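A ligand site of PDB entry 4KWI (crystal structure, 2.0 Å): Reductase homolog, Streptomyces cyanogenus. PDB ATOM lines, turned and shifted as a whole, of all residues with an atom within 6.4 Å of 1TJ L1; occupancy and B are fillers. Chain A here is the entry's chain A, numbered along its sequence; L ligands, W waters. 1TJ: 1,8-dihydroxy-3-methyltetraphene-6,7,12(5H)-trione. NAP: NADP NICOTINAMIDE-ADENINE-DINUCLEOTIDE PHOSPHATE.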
ATOM      1  N   MET A 111      10.771 -16.392 -29.010  1.00  0.00           N
ATOM      2  CA  MET A 111      11.651 -15.889 -30.056  1.00  0.00           C
ATOM      3  C   MET A 111      10.832 -15.713 -31.348  1.00  0.00           C
ATOM      4  O   MET A 111       9.945 -16.504 -31.635  1.00  0.00           O
ATOM      5  CB  MET A 111      12.812 -16.860 -30.276  1.00  0.00           C
ATOM      6  CG  MET A 111      14.053 -16.206 -30.879  1.00  0.00           C
ATOM      7  SD  MET A 111      15.504 -17.271 -30.759  1.00  0.00           S
ATOM      8  CE  MET A 111      15.371 -18.169 -32.314  1.00  0.00           C
ATOM      9  N   MET A 113      12.212 -14.678 -35.085  1.00  0.00           N
ATOM     10  CA  MET A 113      13.231 -14.258 -36.054  1.00  0.00           C
ATOM     11  C   MET A 113      12.658 -13.664 -37.350  1.00  0.00           C
ATOM     12  O   MET A 113      11.633 -14.131 -37.844  1.00  0.00           O
ATOM     13  CB  MET A 113      14.145 -15.450 -36.373  1.00  0.00           C
ATOM     14  CG  MET A 113      15.084 -15.265 -37.546  1.00  0.00           C
ATOM     15  SD  MET A 113      16.048 -16.763 -37.811  1.00  0.00           S
ATOM     16  CE  MET A 113      14.972 -17.711 -38.892  1.00  0.00           C
ATOM     17  N   SER A 157      20.690 -14.961 -23.108  1.00  0.00           N
ATOM     18  CA  SER A 157      21.129 -15.536 -24.388  1.00  0.00           C
ATOM     19  C   SER A 157      22.450 -14.904 -24.834  1.00  0.00           C
ATOM     20  O   SER A 157      22.666 -13.706 -24.631  1.00  0.00           O
ATOM     21  CB  SER A 157      20.107 -15.257 -25.473  1.00  0.00           C
ATOM     22  OG  SER A 157      20.623 -15.567 -26.760  1.00  0.00           O
ATOM     23  N   GLY A 158      23.316 -15.705 -25.453  1.00  0.00           N
ATOM     24  CA  GLY A 158      24.530 -15.175 -26.100  1.00  0.00           C
ATOM     25  C   GLY A 158      24.258 -14.055 -27.104  1.00  0.00           C
ATOM     26  O   GLY A 158      25.136 -13.237 -27.391  1.00  0.00           O
ATOM     27  N   LEU A 159      23.029 -13.995 -27.616  1.00  0.00           N
ATOM     28  CA  LEU A 159      22.643 -12.944 -28.572  1.00  0.00           C
ATOM     29  C   LEU A 159      22.665 -11.525 -28.017  1.00  0.00           C
ATOM     30  O   LEU A 159      22.491 -10.561 -28.770  1.00  0.00           O
ATOM     31  CB  LEU A 159      21.290 -13.245 -29.222  1.00  0.00           C
ATOM     32  CG  LEU A 159      21.286 -14.333 -30.311  1.00  0.00           C
ATOM     33  CD1 LEU A 159      19.906 -14.930 -30.510  1.00  0.00           C
ATOM     34  CD2 LEU A 159      21.848 -13.857 -31.645  1.00  0.00           C
ATOM     35  N   VAL A 162      26.394 -11.180 -29.377  1.00  0.00           N
ATOM     36  CA  VAL A 162      26.651 -11.489 -30.797  1.00  0.00           C
ATOM     37  C   VAL A 162      25.587 -10.814 -31.679  1.00  0.00           C
ATOM     38  O   VAL A 162      24.399 -11.120 -31.573  1.00  0.00           O
ATOM     39  CB  VAL A 162      26.649 -13.023 -31.057  1.00  0.00           C
ATOM     40  CG1 VAL A 162      26.939 -13.344 -32.525  1.00  0.00           C
ATOM     41  CG2 VAL A 162      27.681 -13.724 -30.176  1.00  0.00           C
ATOM     42  N   SER A 164      23.090  -9.990 -34.464  1.00  0.00           N
ATOM     43  CA  SER A 164      22.284 -10.676 -35.486  1.00  0.00           C
ATOM     44  C   SER A 164      21.038  -9.834 -35.782  1.00  0.00           C
ATOM     45  O   SER A 164      20.108  -9.788 -34.966  1.00  0.00           O
ATOM     46  CB  SER A 164      21.853 -12.088 -35.041  1.00  0.00           C
ATOM     47  OG  SER A 164      22.945 -12.793 -34.463  1.00  0.00           O
ATOM     48  N   GLN A 167      17.480 -10.907 -35.095  1.00  0.00           N
ATOM     49  CA  GLN A 167      17.144 -11.183 -33.699  1.00  0.00           C
ATOM     50  C   GLN A 167      17.155  -9.934 -32.825  1.00  0.00           C
ATOM     51  O   GLN A 167      17.188 -10.032 -31.592  1.00  0.00           O
ATOM     52  CB  GLN A 167      18.139 -12.199 -33.116  1.00  0.00           C
ATOM     53  CG  GLN A 167      18.239 -13.537 -33.845  1.00  0.00           C
ATOM     54  CD  GLN A 167      17.104 -14.486 -33.510  1.00  0.00           C
ATOM     55  OE1 GLN A 167      16.043 -14.063 -33.058  1.00  0.00           O
ATOM     56  NE2 GLN A 167      17.324 -15.771 -33.741  1.00  0.00           N
ATOM     57  N   TYR A 170      14.499  -9.569 -30.024  1.00  0.00           N
ATOM     58  CA  TYR A 170      14.864 -10.598 -29.046  1.00  0.00           C
ATOM     59  C   TYR A 170      16.054 -10.125 -28.195  1.00  0.00           C
ATOM     60  O   TYR A 170      15.995 -10.165 -26.971  1.00  0.00           O
ATOM     61  CB  TYR A 170      15.189 -11.893 -29.751  1.00  0.00           C
ATOM     62  CG  TYR A 170      15.620 -13.002 -28.821  1.00  0.00           C
ATOM     63  CD1 TYR A 170      14.693 -13.848 -28.227  1.00  0.00           C
ATOM     64  CD2 TYR A 170      16.976 -13.213 -28.543  1.00  0.00           C
ATOM     65  CE1 TYR A 170      15.093 -14.868 -27.373  1.00  0.00           C
ATOM     66  CE2 TYR A 170      17.385 -14.231 -27.700  1.00  0.00           C
ATOM     67  CZ  TYR A 170      16.440 -15.055 -27.116  1.00  0.00           C
ATOM     68  OH  TYR A 170      16.827 -16.077 -26.272  1.00  0.00           O
ATOM     69  N   ALA A 199      23.564 -17.179 -19.772  1.00  0.00           N
ATOM     70  CA  ALA A 199      23.461 -17.078 -21.219  1.00  0.00           C
ATOM     71  C   ALA A 199      23.852 -18.386 -21.893  1.00  0.00           C
ATOM     72  O   ALA A 199      25.019 -18.661 -22.078  1.00  0.00           O
ATOM     73  CB  ALA A 199      24.311 -15.930 -21.745  1.00  0.00           C
ATOM     74  N   PRO A 200      22.866 -19.198 -22.284  1.00  0.00           N
ATOM     75  CA  PRO A 200      23.183 -20.363 -23.104  1.00  0.00           C
ATOM     76  C   PRO A 200      23.565 -19.959 -24.512  1.00  0.00           C
ATOM     77  O   PRO A 200      23.249 -18.852 -24.963  1.00  0.00           O
ATOM     78  CB  PRO A 200      21.858 -21.148 -23.160  1.00  0.00           C
ATOM     79  CG  PRO A 200      20.905 -20.418 -22.259  1.00  0.00           C
ATOM     80  CD  PRO A 200      21.417 -19.026 -22.121  1.00  0.00           C
ATOM     81  N   GLY A 201      24.270 -20.842 -25.200  1.00  0.00           N
ATOM     82  CA  GLY A 201      24.397 -20.713 -26.638  1.00  0.00           C
ATOM     83  C   GLY A 201      23.265 -21.506 -27.253  1.00  0.00           C
ATOM     84  O   GLY A 201      22.286 -21.842 -26.573  1.00  0.00           O
ATOM     85  N   SER A 202      23.400 -21.818 -28.534  1.00  0.00           N
ATOM     86  CA  SER A 202      22.444 -22.652 -29.243  1.00  0.00           C
ATOM     87  C   SER A 202      22.267 -23.986 -28.525  1.00  0.00           C
ATOM     88  O   SER A 202      23.233 -24.719 -28.302  1.00  0.00           O
ATOM     89  CB  SER A 202      22.922 -22.874 -30.681  1.00  0.00           C
ATOM     90  OG  SER A 202      21.931 -23.519 -31.456  1.00  0.00           O
ATOM     91  N   THR A 203      21.017 -24.288 -28.170  1.00  0.00           N
ATOM     92  CA  THR A 203      20.682 -25.446 -27.363  1.00  0.00           C
ATOM     93  C   THR A 203      19.505 -26.192 -27.979  1.00  0.00           C
ATOM     94  O   THR A 203      18.463 -25.589 -28.257  1.00  0.00           O
ATOM     95  CB  THR A 203      20.295 -25.014 -25.928  1.00  0.00           C
ATOM     96  OG1 THR A 203      21.336 -24.199 -25.371  1.00  0.00           O
ATOM     97  CG2 THR A 203      20.043 -26.223 -25.029  1.00  0.00           C
ATOM     98  N   LEU A 209      12.963 -27.746 -35.387  1.00  0.00           N
ATOM     99  CA  LEU A 209      13.997 -26.857 -35.930  1.00  0.00           C
ATOM    100  C   LEU A 209      15.413 -27.461 -35.877  1.00  0.00           C
ATOM    101  O   LEU A 209      16.143 -27.425 -36.871  1.00  0.00           O
ATOM    102  CB  LEU A 209      13.947 -25.515 -35.189  1.00  0.00           C
ATOM    103  CG  LEU A 209      15.100 -24.508 -35.352  1.00  0.00           C
ATOM    104  CD1 LEU A 209      14.933 -23.679 -36.615  1.00  0.00           C
ATOM    105  CD2 LEU A 209      15.165 -23.615 -34.116  1.00  0.00           C
ATOM    106  N   PHE A 210      15.782 -28.024 -34.715  1.00  0.00           N
ATOM    107  CA  PHE A 210      17.145 -28.552 -34.479  1.00  0.00           C
ATOM    108  C   PHE A 210      17.412 -29.915 -35.112  1.00  0.00           C
ATOM    109  O   PHE A 210      18.487 -30.493 -34.922  1.00  0.00           O
ATOM    110  CB  PHE A 210      17.434 -28.610 -32.967  1.00  0.00           C
ATOM    111  CG  PHE A 210      17.633 -27.259 -32.340  1.00  0.00           C
ATOM    112  CD1 PHE A 210      16.550 -26.538 -31.859  1.00  0.00           C
ATOM    113  CD2 PHE A 210      18.907 -26.723 -32.228  1.00  0.00           C
ATOM    114  CE1 PHE A 210      16.733 -25.289 -31.274  1.00  0.00           C
ATOM    115  CE2 PHE A 210      19.090 -25.479 -31.652  1.00  0.00           C
ATOM    116  CZ  PHE A 210      18.007 -24.761 -31.181  1.00  0.00           C
ATOM    117  N   VAL A 215      20.309 -26.533 -40.702  1.00  0.00           N
ATOM    118  CA  VAL A 215      20.162 -25.595 -39.585  1.00  0.00           C
ATOM    119  C   VAL A 215      21.060 -26.039 -38.408  1.00  0.00           C
ATOM    120  O   VAL A 215      21.715 -25.211 -37.776  1.00  0.00           O
ATOM    121  CB  VAL A 215      18.689 -25.441 -39.139  1.00  0.00           C
ATOM    122  CG1 VAL A 215      18.578 -24.492 -37.948  1.00  0.00           C
ATOM    123  CG2 VAL A 215      17.831 -24.936 -40.287  1.00  0.00           C
ATOM    124  N   LEU A 219      24.247 -23.892 -36.742  1.00  0.00           N
ATOM    125  CA  LEU A 219      24.206 -23.653 -35.292  1.00  0.00           C
ATOM    126  C   LEU A 219      25.332 -24.343 -34.543  1.00  0.00           C
ATOM    127  O   LEU A 219      25.821 -23.807 -33.555  1.00  0.00           O
ATOM    128  CB  LEU A 219      22.845 -24.026 -34.701  1.00  0.00           C
ATOM    129  CG  LEU A 219      21.608 -23.275 -35.197  1.00  0.00           C
ATOM    130  CD1 LEU A 219      20.360 -23.819 -34.524  1.00  0.00           C
ATOM    131  CD2 LEU A 219      21.740 -21.769 -34.984  1.00  0.00           C
ATOM    132  N   LEU A 222      28.684 -22.305 -34.271  1.00  0.00           N
ATOM    133  CA  LEU A 222      28.771 -21.150 -33.351  1.00  0.00           C
ATOM    134  C   LEU A 222      29.613 -21.409 -32.096  1.00  0.00           C
ATOM    135  O   LEU A 222      30.341 -20.532 -31.626  1.00  0.00           O
ATOM    136  CB  LEU A 222      27.376 -20.689 -32.942  1.00  0.00           C
ATOM    137  CG  LEU A 222      26.466 -20.076 -34.009  1.00  0.00           C
ATOM    138  CD1 LEU A 222      25.009 -20.069 -33.552  1.00  0.00           C
ATOM    139  CD2 LEU A 222      26.915 -18.664 -34.344  1.00  0.00           C
ATOM    140  N   SER A 257      27.739 -20.808 -22.947  1.00  0.00           N
ATOM    141  CA  SER A 257      27.506 -20.878 -24.388  1.00  0.00           C
ATOM    142  C   SER A 257      28.440 -21.837 -25.108  1.00  0.00           C
ATOM    143  O   SER A 257      28.346 -21.994 -26.338  1.00  0.00           O
ATOM    144  CB  SER A 257      27.639 -19.484 -25.025  1.00  0.00           C
ATOM    145  OG  SER A 257      29.000 -19.096 -25.107  1.00  0.00           O
ATOM    146  N   THR A 260      30.829 -19.628 -27.529  1.00  0.00           N
ATOM    147  CA  THR A 260      30.179 -18.917 -28.629  1.00  0.00           C
ATOM    148  C   THR A 260      30.562 -17.440 -28.666  1.00  0.00           C
ATOM    149  O   THR A 260      30.506 -16.798 -29.708  1.00  0.00           O
ATOM    150  CB  THR A 260      28.651 -19.102 -28.560  1.00  0.00           C
ATOM    151  OG1 THR A 260      28.336 -20.494 -28.657  1.00  0.00           O
ATOM    152  CG2 THR A 260      27.937 -18.366 -29.696  1.00  0.00           C
ATOM    153  N   LEU A 261      30.934 -16.902 -27.509  1.00  0.00           N
ATOM    154  CA  LEU A 261      31.207 -15.483 -27.316  1.00  0.00           C
ATOM    155  C   LEU A 261      32.710 -15.157 -27.395  1.00  0.00           C
ATOM    156  O   LEU A 261      33.174 -14.238 -26.736  1.00  0.00           O
ATOM    157  CB  LEU A 261      30.602 -14.990 -25.984  1.00  0.00           C
ATOM    158  CG  LEU A 261      29.133 -15.404 -25.721  1.00  0.00           C
ATOM    159  CD1 LEU A 261      28.629 -14.988 -24.350  1.00  0.00           C
ATOM    160  CD2 LEU A 261      28.176 -14.886 -26.790  1.00  0.00           C
HETATM  161  OAD 1TJ L   1      22.075 -17.481 -33.903  1.00  0.00           O
HETATM  162  CAV 1TJ L   1      21.914 -17.807 -32.729  1.00  0.00           C
HETATM  163  CAT 1TJ L   1      20.791 -18.551 -32.333  1.00  0.00           C
HETATM  164  CAS 1TJ L   1      19.752 -18.978 -33.198  1.00  0.00           C
HETATM  165  CAO 1TJ L   1      19.397 -18.316 -34.382  1.00  0.00           C
HETATM  166  OAE 1TJ L   1      20.125 -17.218 -34.749  1.00  0.00           O
HETATM  167  CAJ 1TJ L   1      18.357 -18.755 -35.187  1.00  0.00           C
HETATM  168  CAN 1TJ L   1      17.612 -19.878 -34.810  1.00  0.00           C
HETATM  169  CAA 1TJ L   1      16.566 -20.314 -35.627  1.00  0.00           C
HETATM  170  CAK 1TJ L   1      17.921 -20.542 -33.615  1.00  0.00           C
HETATM  171  CAQ 1TJ L   1      18.977 -20.093 -32.815  1.00  0.00           C
HETATM  172  CAL 1TJ L   1      19.282 -20.725 -31.602  1.00  0.00           C
HETATM  173  CAM 1TJ L   1      19.503 -19.667 -30.709  1.00  0.00           C
HETATM  174  OAB 1TJ L   1      18.668 -19.356 -29.877  1.00  0.00           O
HETATM  175  CAR 1TJ L   1      20.644 -18.903 -30.982  1.00  0.00           C
HETATM  176  CAU 1TJ L   1      21.587 -18.533 -30.019  1.00  0.00           C
HETATM  177  OAC 1TJ L   1      21.439 -18.857 -28.834  1.00  0.00           O
HETATM  178  CAX 1TJ L   1      22.718 -17.784 -30.417  1.00  0.00           C
HETATM  179  CAW 1TJ L   1      22.865 -17.432 -31.768  1.00  0.00           C
HETATM  180  CAI 1TJ L   1      23.988 -16.693 -32.173  1.00  0.00           C
HETATM  181  CAG 1TJ L   1      24.948 -16.292 -31.256  1.00  0.00           C
HETATM  182  CAH 1TJ L   1      24.811 -16.630 -29.922  1.00  0.00           C
HETATM  183  CAP 1TJ L   1      23.708 -17.378 -29.512  1.00  0.00           C
HETATM  184  OAF 1TJ L   1      23.555 -17.702 -28.207  1.00  0.00           O
HETATM  185  PA  NAP L   2      11.309 -23.248 -26.040  1.00  0.00           P
HETATM  186  O1A NAP L   2      10.906 -24.729 -26.090  1.00  0.00           O
HETATM  187  O2A NAP L   2      10.304 -22.300 -26.604  1.00  0.00           O
HETATM  188  O5B NAP L   2      10.346 -23.362 -24.680  1.00  0.00           O
HETATM  189  C5B NAP L   2       9.522 -22.269 -24.181  1.00  0.00           C
HETATM  190  C4B NAP L   2       8.950 -22.506 -22.736  1.00  0.00           C
HETATM  191  O4B NAP L   2       8.478 -21.262 -22.201  1.00  0.00           O
HETATM  192  C3B NAP L   2       7.711 -23.413 -22.733  1.00  0.00           C
HETATM  193  O3B NAP L   2       7.606 -24.052 -21.447  1.00  0.00           O
HETATM  194  C2B NAP L   2       6.553 -22.460 -22.921  1.00  0.00           C
HETATM  195  O2B NAP L   2       5.348 -22.942 -22.306  1.00  0.00           O
HETATM  196  C1B NAP L   2       7.021 -21.265 -22.101  1.00  0.00           C
HETATM  197  N9A NAP L   2       6.356 -19.977 -22.562  1.00  0.00           N
HETATM  198  C8A NAP L   2       6.487 -19.391 -23.745  1.00  0.00           C
HETATM  199  N7A NAP L   2       5.745 -18.283 -23.743  1.00  0.00           N
HETATM  200  C5A NAP L   2       5.129 -18.178 -22.566  1.00  0.00           C
HETATM  201  C6A NAP L   2       4.281 -17.263 -22.053  1.00  0.00           C
HETATM  202  N6A NAP L   2       3.935 -16.225 -22.847  1.00  0.00           N
HETATM  203  N1A NAP L   2       3.783 -17.360 -20.811  1.00  0.00           N
HETATM  204  C2A NAP L   2       4.175 -18.452 -20.034  1.00  0.00           C
HETATM  205  N3A NAP L   2       5.058 -19.395 -20.577  1.00  0.00           N
HETATM  206  C4A NAP L   2       5.522 -19.232 -21.828  1.00  0.00           C
HETATM  207  O3  NAP L   2      12.332 -22.673 -24.902  1.00  0.00           O
HETATM  208  PN  NAP L   2      13.894 -22.975 -24.925  1.00  0.00           P
HETATM  209  O1N NAP L   2      14.387 -23.036 -26.314  1.00  0.00           O
HETATM  210  O2N NAP L   2      14.094 -24.148 -24.054  1.00  0.00           O
HETATM  211  O5D NAP L   2      14.464 -21.685 -24.220  1.00  0.00           O
HETATM  212  C5D NAP L   2      14.108 -21.343 -22.853  1.00  0.00           C
HETATM  213  C4D NAP L   2      14.817 -20.023 -22.485  1.00  0.00           C
HETATM  214  O4D NAP L   2      16.222 -20.076 -22.837  1.00  0.00           O
HETATM  215  C3D NAP L   2      14.217 -18.826 -23.265  1.00  0.00           C
HETATM  216  O3D NAP L   2      14.272 -17.680 -22.397  1.00  0.00           O
HETATM  217  C2D NAP L   2      15.135 -18.623 -24.425  1.00  0.00           C
HETATM  218  O2D NAP L   2      15.185 -17.230 -24.813  1.00  0.00           O
HETATM  219  C1D NAP L   2      16.490 -19.030 -23.816  1.00  0.00           C
HETATM  220  N1N NAP L   2      17.475 -19.511 -24.795  1.00  0.00           N
HETATM  221  C2N NAP L   2      17.243 -20.628 -25.650  1.00  0.00           C
HETATM  222  C3N NAP L   2      18.264 -21.031 -26.531  1.00  0.00           C
HETATM  223  C7N NAP L   2      18.126 -22.113 -27.409  1.00  0.00           C
HETATM  224  O7N NAP L   2      18.923 -22.277 -28.332  1.00  0.00           O
HETATM  225  N7N NAP L   2      17.094 -22.945 -27.178  1.00  0.00           N
HETATM  226  C4N NAP L   2      19.473 -20.321 -26.545  1.00  0.00           C
HETATM  227  C5N NAP L   2      19.709 -19.231 -25.699  1.00  0.00           C
HETATM  228  C6N NAP L   2      18.724 -18.826 -24.818  1.00  0.00           C
HETATM  229  P2B NAP L   2       4.318 -23.942 -23.065  1.00  0.00           P
HETATM  230  O1X NAP L   2       2.985 -23.866 -22.193  1.00  0.00           O
HETATM  231  O2X NAP L   2       3.973 -23.207 -24.447  1.00  0.00           O
HETATM  232  O3X NAP L   2       4.901 -25.285 -23.198  1.00  0.00           O
HETATM  233  O   HOH W   1      18.827 -17.318 -28.091  1.00  0.00           O
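O of Pro 200 lies within hydrogen-bond range of OAF of 1TJ L1, at 3.5 Å.
The backbone NH (N) of Gly 158 is in hydrogen-bond range of an oxygen (OAF) of 1TJ L1 (3.4 Å).
An oxygen (O2D) of NAP L2 lies within hydrogen-bond range of the side-chain hydroxyl of Tyr 170.
The backbone carbonyl oxygen (O) of Thr 203 lies within hydrogen-bond range of a nitrogen (N7N) of NAP L2.
N of Thr 203 is in hydrogen-bond range of O7N of NAP L2 (2.9 Å).
OAE of 1TJ L1 lies within hydrogen-bond range of NE2 of Gln 167, at 3.3 Å.
The backbone carbonyl oxygen of Gly 201 sits at hydrogen-bond distance from the side-chain hydroxyl of Thr 203.
OG1 of Thr 260 is in hydrogen-bond range of O of Ser 257 (2.8 Å).
The backbone NH of Leu 159 sits close to the side-chain hydroxyl of Ser 157 (3.0 Å).
The backbone carbonyl oxygen (O) of Pro 200 lies within hydrogen-bond range of the backbone NH (N) of Gly 158 (3.2 Å).
Met 111 touches 1TJ L1 (CE to CAK, 3.7 Å).
OG of Ser 157 touches OAF of 1TJ L1, 3.9 Å away.
Leu 159 touches 1TJ L1 (CD2 to CAI, 3.6 Å).
Val 162 touches 1TJ L1 (CB to CAG, 3.7 Å).
CA of Gly 201 touches OAF of 1TJ L1, at 3.5 Å.
Ser 202 touches 1TJ L1.
Leu 209 touches 1TJ L1 (CD1 to CAA, 3.9 Å).
Leu 219 touches 1TJ L1.
Leu 222 touches 1TJ L1 (CD1 to CAI, 3.8 Å).
Thr 260 touches 1TJ L1.
Hydrophobic or aromatic side chains within 4 Å of 1TJ L1: Met 111, Leu 159, Val 162, Leu 209, Leu 219 and Leu 222.
Within 4 Å of 1TJ L1: Met 111, Ser 157, Gly 158, Leu 159, Val 162, Gln 167, Pro 200, Gly 201, Ser 202, Leu 209, Leu 219, Leu 222 and Thr 260.
The nearest printed residue that does not touch 1TJ L1 is Met 113 (4.02 Å).
Water W1 lies within hydrogen-bond range of OAB of 1TJ L1 (2.7 Å), OG of Ser 157 (2.8 Å) and OH of Tyr 170 (3.0 Å).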
